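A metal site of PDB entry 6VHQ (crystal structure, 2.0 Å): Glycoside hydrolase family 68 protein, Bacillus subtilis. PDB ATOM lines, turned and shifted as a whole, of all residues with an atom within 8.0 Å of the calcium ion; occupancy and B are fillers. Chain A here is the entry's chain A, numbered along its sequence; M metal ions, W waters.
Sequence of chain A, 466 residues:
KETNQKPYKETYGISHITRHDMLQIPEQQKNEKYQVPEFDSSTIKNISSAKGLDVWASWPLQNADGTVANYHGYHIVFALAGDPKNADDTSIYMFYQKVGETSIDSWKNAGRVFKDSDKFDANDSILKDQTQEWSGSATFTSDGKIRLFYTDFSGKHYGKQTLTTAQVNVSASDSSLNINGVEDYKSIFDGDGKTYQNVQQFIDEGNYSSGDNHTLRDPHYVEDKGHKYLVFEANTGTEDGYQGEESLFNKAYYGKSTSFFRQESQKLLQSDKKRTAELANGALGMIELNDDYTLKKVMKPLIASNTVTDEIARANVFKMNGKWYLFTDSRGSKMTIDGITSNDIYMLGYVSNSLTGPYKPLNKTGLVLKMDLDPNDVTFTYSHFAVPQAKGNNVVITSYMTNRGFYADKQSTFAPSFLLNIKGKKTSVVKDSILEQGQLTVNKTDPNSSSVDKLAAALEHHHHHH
Five residues have an atom within 4 Å of the calcium ion: Asp 212, Gln 243, Leu 279, Asn 281 and Asp 310.
The nearest printed residue that does not touch the calcium ion is Asn 235 (4.2 Å).
The calcium ion is bound by the backbone carbonyl oxygen (O) of Leu 279 (2.3 Å), the side-chain amide oxygen (OE1) of Gln 243 (2.3 Å), the side-chain carboxylate (OD1) of Asp 212 (2.3 Å), the side-chain amide oxygen (OD1) of Asn 281 (2.4 Å), water W1 (2.4 Å), the side-chain carboxylate (OD2) of Asp 310 (2.6 Å) and the side-chain carboxylate (OD1) of Asp 310 (2.6 Å).
Water W1 lies within hydrogen-bond range of the side-chain amide oxygen (OE1) of Gln 197 (2.7 Å), the backbone carbonyl oxygen (O) of Asn 213 (2.9 Å) and the side-chain amide nitrogen (ND2) of Asn 235 (3.3 Å).
The side-chain amide oxygen (OD1) of Asn 281 lies close to the side-chain amide nitrogen (ND2) of Asn 235, 3.5 Å away.
OD2 of Asp 310 lies close to N of Asn 213 (2.9 Å).
The side-chain carboxylate (OE2) of Glu 205 sits close to the side-chain carboxylate (OD2) of Asp 212 (2.5 Å).
The side-chain carboxylate (OD2) of Asp 212 sits at hydrogen-bond distance from the side-chain amide nitrogen (NE2) of Gln 197, 3.2 Å away.
The backbone carbonyl oxygen (O) of Asp 310 sits at hydrogen-bond distance from the side-chain amide nitrogen (ND2) of Asn 235 (3.0 Å).
OG of Ser 210 sits at hydrogen-bond distance from N of Asp 212 (3.1 Å).
The side-chain amide nitrogen (NE2) of Gln 243 sits at hydrogen-bond distance from the side-chain carboxylate (OE1) of Glu 205, 3.0 Å away.
The side-chain amide nitrogen (ND2) of Asn 281 lies within hydrogen-bond range of the side-chain hydroxyl (OG1) of Thr 236.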
ATOM      1  N   GLN A 197      14.594  19.451 -24.163  1.00  0.00           N
ATOM      2  CA  GLN A 197      13.223  19.036 -24.401  1.00  0.00           C
ATOM      3  C   GLN A 197      12.338  20.268 -24.548  1.00  0.00           C
ATOM      4  O   GLN A 197      12.533  21.258 -23.843  1.00  0.00           O
ATOM      5  CB  GLN A 197      12.737  18.177 -23.238  1.00  0.00           C
ATOM      6  CG  GLN A 197      11.425  17.359 -23.552  1.00  0.00           C
ATOM      7  CD  GLN A 197      10.976  16.559 -22.344  1.00  0.00           C
ATOM      8  OE1 GLN A 197      10.808  17.110 -21.251  1.00  0.00           O
ATOM      9  NE2 GLN A 197      10.806  15.265 -22.514  1.00  0.00           N
ATOM     10  N   PHE A 202       6.639  16.720 -24.281  1.00  0.00           N
ATOM     11  CA  PHE A 202       5.894  16.413 -23.064  1.00  0.00           C
ATOM     12  C   PHE A 202       4.438  16.124 -23.374  1.00  0.00           C
ATOM     13  O   PHE A 202       3.864  15.123 -22.888  1.00  0.00           O
ATOM     14  CB  PHE A 202       6.014  17.588 -22.038  1.00  0.00           C
ATOM     15  CG  PHE A 202       5.277  17.333 -20.731  1.00  0.00           C
ATOM     16  CD1 PHE A 202       5.633  16.274 -19.909  1.00  0.00           C
ATOM     17  CD2 PHE A 202       4.226  18.139 -20.331  1.00  0.00           C
ATOM     18  CE1 PHE A 202       4.962  16.023 -18.682  1.00  0.00           C
ATOM     19  CE2 PHE A 202       3.591  17.897 -19.100  1.00  0.00           C
ATOM     20  CZ  PHE A 202       3.962  16.826 -18.289  1.00  0.00           C
ATOM     21  N   GLU A 205       3.749  12.769 -25.599  1.00  0.00           N
ATOM     22  CA  GLU A 205       4.011  11.474 -24.956  1.00  0.00           C
ATOM     23  C   GLU A 205       2.966  11.159 -23.886  1.00  0.00           C
ATOM     24  O   GLU A 205       3.015  10.074 -23.286  1.00  0.00           O
ATOM     25  CB  GLU A 205       5.389  11.455 -24.311  1.00  0.00           C
ATOM     26  CG  GLU A 205       5.422  12.432 -23.164  1.00  0.00           C
ATOM     27  CD  GLU A 205       6.798  12.629 -22.471  1.00  0.00           C
ATOM     28  OE1 GLU A 205       7.694  11.787 -22.589  1.00  0.00           O
ATOM     29  OE2 GLU A 205       6.956  13.640 -21.749  1.00  0.00           O
ATOM     30  N   SER A 210       2.085  10.527 -18.031  1.00  0.00           N
ATOM     31  CA  SER A 210       3.225   9.711 -18.415  1.00  0.00           C
ATOM     32  C   SER A 210       4.240   9.545 -17.304  1.00  0.00           C
ATOM     33  O   SER A 210       5.123   8.696 -17.422  1.00  0.00           O
ATOM     34  CB  SER A 210       3.951  10.305 -19.617  1.00  0.00           C
ATOM     35  OG  SER A 210       4.595  11.542 -19.249  1.00  0.00           O
ATOM     36  N   GLY A 211       4.187  10.381 -16.273  1.00  0.00           N
ATOM     37  CA  GLY A 211       5.193  10.405 -15.243  1.00  0.00           C
ATOM     38  C   GLY A 211       6.414  11.233 -15.594  1.00  0.00           C
ATOM     39  O   GLY A 211       7.303  11.380 -14.733  1.00  0.00           O
ATOM     40  N   ASP A 212       6.491  11.746 -16.818  1.00  0.00           N
ATOM     41  CA  ASP A 212       7.587  12.615 -17.203  1.00  0.00           C
ATOM     42  C   ASP A 212       7.456  13.972 -16.491  1.00  0.00           C
ATOM     43  O   ASP A 212       6.362  14.377 -16.138  1.00  0.00           O
ATOM     44  CB  ASP A 212       7.602  12.776 -18.716  1.00  0.00           C
ATOM     45  CG  ASP A 212       8.965  13.188 -19.251  1.00  0.00           C
ATOM     46  OD1 ASP A 212       9.966  13.077 -18.549  1.00  0.00           O
ATOM     47  OD2 ASP A 212       9.028  13.642 -20.385  1.00  0.00           O
ATOM     48  N   ASN A 213       8.575  14.646 -16.258  1.00  0.00           N
ATOM     49  CA  ASN A 213       8.581  15.957 -15.596  1.00  0.00           C
ATOM     50  C   ASN A 213       9.332  16.921 -16.522  1.00  0.00           C
ATOM     51  O   ASN A 213      10.569  16.965 -16.494  1.00  0.00           O
ATOM     52  CB  ASN A 213       9.274  15.863 -14.216  1.00  0.00           C
ATOM     53  CG  ASN A 213       9.341  17.194 -13.492  1.00  0.00           C
ATOM     54  OD1 ASN A 213       8.789  18.202 -13.943  1.00  0.00           O
ATOM     55  ND2 ASN A 213      10.017  17.199 -12.314  1.00  0.00           N
ATOM     56  N   HIS A 214       8.581  17.705 -17.325  1.00  0.00           N
ATOM     57  CA  HIS A 214       9.200  18.628 -18.265  1.00  0.00           C
ATOM     58  C   HIS A 214       9.508  19.947 -17.574  1.00  0.00           C
ATOM     59  O   HIS A 214       8.649  20.519 -16.885  1.00  0.00           O
ATOM     60  CB  HIS A 214       8.287  18.873 -19.474  1.00  0.00           C
ATOM     61  CG  HIS A 214       8.777  19.990 -20.318  1.00  0.00           C
ATOM     62  ND1 HIS A 214       9.925  19.893 -21.055  1.00  0.00           N
ATOM     63  CD2 HIS A 214       8.336  21.257 -20.470  1.00  0.00           C
ATOM     64  CE1 HIS A 214      10.157  21.047 -21.668  1.00  0.00           C
ATOM     65  NE2 HIS A 214       9.198  21.893 -21.329  1.00  0.00           N
ATOM     66  N   THR A 215      10.732  20.459 -17.798  1.00  0.00           N
ATOM     67  CA  THR A 215      11.190  21.684 -17.126  1.00  0.00           C
ATOM     68  C   THR A 215      11.970  22.549 -18.106  1.00  0.00           C
ATOM     69  O   THR A 215      12.702  22.051 -18.981  1.00  0.00           O
ATOM     70  CB  THR A 215      12.067  21.362 -15.900  1.00  0.00           C
ATOM     71  OG1 THR A 215      13.399  21.030 -16.326  1.00  0.00           O
ATOM     72  CG2 THR A 215      11.526  20.154 -15.062  1.00  0.00           C
ATOM     73  N   ALA A 234      16.764  22.447 -17.279  1.00  0.00           N
ATOM     74  CA  ALA A 234      16.085  21.936 -18.437  1.00  0.00           C
ATOM     75  C   ALA A 234      16.098  20.409 -18.383  1.00  0.00           C
ATOM     76  O   ALA A 234      16.414  19.814 -17.366  1.00  0.00           O
ATOM     77  CB  ALA A 234      16.735  22.479 -19.706  1.00  0.00           C
ATOM     78  N   ASN A 235      15.722  19.784 -19.503  1.00  0.00           N
ATOM     79  CA  ASN A 235      15.870  18.352 -19.730  1.00  0.00           C
ATOM     80  C   ASN A 235      16.553  18.115 -21.088  1.00  0.00           C
ATOM     81  O   ASN A 235      16.395  18.923 -21.998  1.00  0.00           O
ATOM     82  CB  ASN A 235      14.489  17.667 -19.699  1.00  0.00           C
ATOM     83  CG  ASN A 235      13.806  17.890 -18.380  1.00  0.00           C
ATOM     84  OD1 ASN A 235      13.122  18.887 -18.218  1.00  0.00           O
ATOM     85  ND2 ASN A 235      14.122  17.041 -17.368  1.00  0.00           N
ATOM     86  N   THR A 236      17.265  17.007 -21.227  1.00  0.00           N
ATOM     87  CA  THR A 236      17.967  16.793 -22.496  1.00  0.00           C
ATOM     88  C   THR A 236      16.960  16.584 -23.640  1.00  0.00           C
ATOM     89  O   THR A 236      15.783  16.345 -23.419  1.00  0.00           O
ATOM     90  CB  THR A 236      18.917  15.577 -22.390  1.00  0.00           C
ATOM     91  OG1 THR A 236      18.143  14.418 -22.074  1.00  0.00           O
ATOM     92  CG2 THR A 236      19.993  15.797 -21.303  1.00  0.00           C
ATOM     93  N   TYR A 242      18.831  11.422 -24.628  1.00  0.00           N
ATOM     94  CA  TYR A 242      17.426  11.524 -24.317  1.00  0.00           C
ATOM     95  C   TYR A 242      17.014  10.493 -23.275  1.00  0.00           C
ATOM     96  O   TYR A 242      17.639   9.440 -23.128  1.00  0.00           O
ATOM     97  CB  TYR A 242      16.589  11.353 -25.599  1.00  0.00           C
ATOM     98  CG  TYR A 242      15.228  12.031 -25.414  1.00  0.00           C
ATOM     99  CD1 TYR A 242      15.141  13.277 -24.725  1.00  0.00           C
ATOM    100  CD2 TYR A 242      14.058  11.470 -25.922  1.00  0.00           C
ATOM    101  CE1 TYR A 242      13.892  13.950 -24.534  1.00  0.00           C
ATOM    102  CE2 TYR A 242      12.835  12.102 -25.743  1.00  0.00           C
ATOM    103  CZ  TYR A 242      12.772  13.375 -25.015  1.00  0.00           C
ATOM    104  OH  TYR A 242      11.538  13.984 -24.862  1.00  0.00           O
ATOM    105  N   GLN A 243      15.934  10.804 -22.543  1.00  0.00           N
ATOM    106  CA  GLN A 243      15.263   9.832 -21.666  1.00  0.00           C
ATOM    107  C   GLN A 243      14.884   8.601 -22.474  1.00  0.00           C
ATOM    108  O   GLN A 243      14.806   8.680 -23.709  1.00  0.00           O
ATOM    109  CB  GLN A 243      13.995  10.420 -21.067  1.00  0.00           C
ATOM    110  CG  GLN A 243      13.032  10.946 -22.142  1.00  0.00           C
ATOM    111  CD  GLN A 243      11.921  11.751 -21.537  1.00  0.00           C
ATOM    112  OE1 GLN A 243      12.178  12.545 -20.657  1.00  0.00           O
ATOM    113  NE2 GLN A 243      10.669  11.538 -22.002  1.00  0.00           N
ATOM    114  N   GLY A 244      14.605   7.482 -21.796  1.00  0.00           N
ATOM    115  CA  GLY A 244      14.041   6.308 -22.452  1.00  0.00           C
ATOM    116  C   GLY A 244      14.745   5.040 -21.954  1.00  0.00           C
ATOM    117  O   GLY A 244      15.689   5.128 -21.142  1.00  0.00           O
ATOM    118  N   ARG A 275      11.168   2.830 -14.602  1.00  0.00           N
ATOM    119  CA  ARG A 275      10.576   3.827 -15.503  1.00  0.00           C
ATOM    120  C   ARG A 275      10.911   5.256 -15.076  1.00  0.00           C
ATOM    121  O   ARG A 275      11.155   6.112 -15.924  1.00  0.00           O
ATOM    122  CB  ARG A 275       9.060   3.606 -15.556  1.00  0.00           C
ATOM    123  CG  ARG A 275       8.344   4.470 -16.594  1.00  0.00           C
ATOM    124  CD  ARG A 275       8.995   4.352 -17.930  1.00  0.00           C
ATOM    125  NE  ARG A 275       8.315   5.132 -18.977  1.00  0.00           N
ATOM    126  CZ  ARG A 275       8.799   5.283 -20.216  1.00  0.00           C
ATOM    127  NH1 ARG A 275       9.944   4.702 -20.564  1.00  0.00           N
ATOM    128  NH2 ARG A 275       8.154   6.018 -21.124  1.00  0.00           N
ATOM    129  N   THR A 276      10.917   5.534 -13.767  1.00  0.00           N
ATOM    130  CA  THR A 276      11.309   6.829 -13.223  1.00  0.00           C
ATOM    131  C   THR A 276      12.739   7.185 -13.633  1.00  0.00           C
ATOM    132  O   THR A 276      13.052   8.338 -13.993  1.00  0.00           O
ATOM    133  CB  THR A 276      11.212   6.827 -11.679  1.00  0.00           C
ATOM    134  OG1 THR A 276       9.878   6.490 -11.255  1.00  0.00           O
ATOM    135  CG2 THR A 276      11.540   8.210 -11.158  1.00  0.00           C
ATOM    136  N   ALA A 277      13.619   6.203 -13.561  1.00  0.00           N
ATOM    137  CA  ALA A 277      14.996   6.431 -13.978  1.00  0.00           C
ATOM    138  C   ALA A 277      15.082   6.599 -15.491  1.00  0.00           C
ATOM    139  O   ALA A 277      15.858   7.421 -15.977  1.00  0.00           O
ATOM    140  CB  ALA A 277      15.856   5.261 -13.522  1.00  0.00           C
ATOM    141  N   GLU A 278      14.309   5.804 -16.263  1.00  0.00           N
ATOM    142  CA  GLU A 278      14.279   5.982 -17.723  1.00  0.00           C
ATOM    143  C   GLU A 278      13.871   7.414 -18.076  1.00  0.00           C
ATOM    144  O   GLU A 278      14.505   8.068 -18.902  1.00  0.00           O
ATOM    145  CB  GLU A 278      13.316   4.982 -18.369  1.00  0.00           C
ATOM    146  CG  GLU A 278      13.934   3.608 -18.504  1.00  0.00           C
ATOM    147  CD  GLU A 278      12.959   2.529 -18.911  1.00  0.00           C
ATOM    148  OE1 GLU A 278      11.753   2.802 -19.157  1.00  0.00           O
ATOM    149  OE2 GLU A 278      13.396   1.366 -18.948  1.00  0.00           O
ATOM    150  N   LEU A 279      12.818   7.923 -17.420  1.00  0.00           N
ATOM    151  CA  LEU A 279      12.281   9.253 -17.699  1.00  0.00           C
ATOM    152  C   LEU A 279      13.185  10.379 -17.193  1.00  0.00           C
ATOM    153  O   LEU A 279      13.111  11.501 -17.723  1.00  0.00           O
ATOM    154  CB  LEU A 279      10.872   9.398 -17.094  1.00  0.00           C
ATOM    155  CG  LEU A 279       9.826   8.519 -17.783  1.00  0.00           C
ATOM    156  CD1 LEU A 279       8.468   8.486 -17.085  1.00  0.00           C
ATOM    157  CD2 LEU A 279       9.623   8.978 -19.246  1.00  0.00           C
ATOM    158  N   ALA A 280      14.030  10.085 -16.205  1.00  0.00           N
ATOM    159  CA  ALA A 280      14.916  11.089 -15.613  1.00  0.00           C
ATOM    160  C   ALA A 280      15.985  11.528 -16.601  1.00  0.00           C
ATOM    161  O   ALA A 280      16.886  10.750 -16.961  1.00  0.00           O
ATOM    162  CB  ALA A 280      15.589  10.533 -14.355  1.00  0.00           C
ATOM    163  N   ASN A 281      15.912  12.782 -17.044  1.00  0.00           N
ATOM    164  CA  ASN A 281      16.944  13.319 -17.910  1.00  0.00           C
ATOM    165  C   ASN A 281      17.119  14.820 -17.650  1.00  0.00           C
ATOM    166  O   ASN A 281      17.175  15.631 -18.573  1.00  0.00           O
ATOM    167  CB  ASN A 281      16.652  13.020 -19.377  1.00  0.00           C
ATOM    168  CG  ASN A 281      15.458  13.791 -19.922  1.00  0.00           C
ATOM    169  OD1 ASN A 281      14.506  14.083 -19.182  1.00  0.00           O
ATOM    170  ND2 ASN A 281      15.520  14.141 -21.239  1.00  0.00           N
ATOM    171  N   GLY A 282      17.288  15.199 -16.377  1.00  0.00           N
ATOM    172  CA  GLY A 282      17.525  16.612 -16.064  1.00  0.00           C
ATOM    173  C   GLY A 282      18.832  17.117 -16.659  1.00  0.00           C
ATOM    174  O   GLY A 282      19.732  16.338 -16.975  1.00  0.00           O
ATOM    175  N   ASN A 306      20.818  12.218 -16.224  1.00  0.00           N
ATOM    176  CA  ASN A 306      20.104  11.013 -16.721  1.00  0.00           C
ATOM    177  C   ASN A 306      20.114   9.905 -15.684  1.00  0.00           C
ATOM    178  O   ASN A 306      21.161   9.561 -15.127  1.00  0.00           O
ATOM    179  CB  ASN A 306      20.751  10.432 -18.020  1.00  0.00           C
ATOM    180  CG  ASN A 306      20.625  11.367 -19.249  1.00  0.00           C
ATOM    181  OD1 ASN A 306      21.408  12.309 -19.388  1.00  0.00           O
ATOM    182  ND2 ASN A 306      19.646  11.096 -20.126  1.00  0.00           N
ATOM    183  N   THR A 309      17.602  11.985 -11.874  1.00  0.00           N
ATOM    184  CA  THR A 309      16.449  12.836 -11.590  1.00  0.00           C
ATOM    185  C   THR A 309      16.083  13.636 -12.825  1.00  0.00           C
ATOM    186  O   THR A 309      16.946  13.975 -13.663  1.00  0.00           O
ATOM    187  CB  THR A 309      16.697  13.815 -10.412  1.00  0.00           C
ATOM    188  OG1 THR A 309      15.537  14.653 -10.261  1.00  0.00           O
ATOM    189  CG2 THR A 309      17.882  14.686 -10.698  1.00  0.00           C
ATOM    190  N   ASP A 310      14.814  13.955 -12.907  1.00  0.00           N
ATOM    191  CA  ASP A 310      14.296  14.823 -13.955  1.00  0.00           C
ATOM    192  C   ASP A 310      14.382  16.250 -13.555  1.00  0.00           C
ATOM    193  O   ASP A 310      14.100  17.124 -14.376  1.00  0.00           O
ATOM    194  CB  ASP A 310      12.811  14.500 -14.253  1.00  0.00           C
ATOM    195  CG  ASP A 310      12.522  14.414 -15.776  1.00  0.00           C
ATOM    196  OD1 ASP A 310      13.441  14.753 -16.540  1.00  0.00           O
ATOM    197  OD2 ASP A 310      11.394  13.984 -16.151  1.00  0.00           O
ATOM    198  N   GLU A 311      14.726  16.521 -12.290  1.00  0.00           N
ATOM    199  CA  GLU A 311      14.625  17.900 -11.789  1.00  0.00           C
ATOM    200  C   GLU A 311      15.896  18.334 -11.052  1.00  0.00           C
ATOM    201  O   GLU A 311      16.130  18.004  -9.878  1.00  0.00           O
ATOM    202  CB  GLU A 311      13.361  18.008 -10.926  1.00  0.00           C
ATOM    203  CG  GLU A 311      13.065  19.405 -10.323  1.00  0.00           C
ATOM    204  CD  GLU A 311      11.707  19.398  -9.589  1.00  0.00           C
ATOM    205  OE1 GLU A 311      10.612  19.296 -10.217  1.00  0.00           O
ATOM    206  OE2 GLU A 311      11.779  19.303  -8.357  1.00  0.00           O
HETATM  207 CA    CA M   1      12.269  13.507 -18.536  1.00  0.00          CA
HETATM  208  O   HOH W   1      11.522  15.745 -18.995  1.00  0.00           O
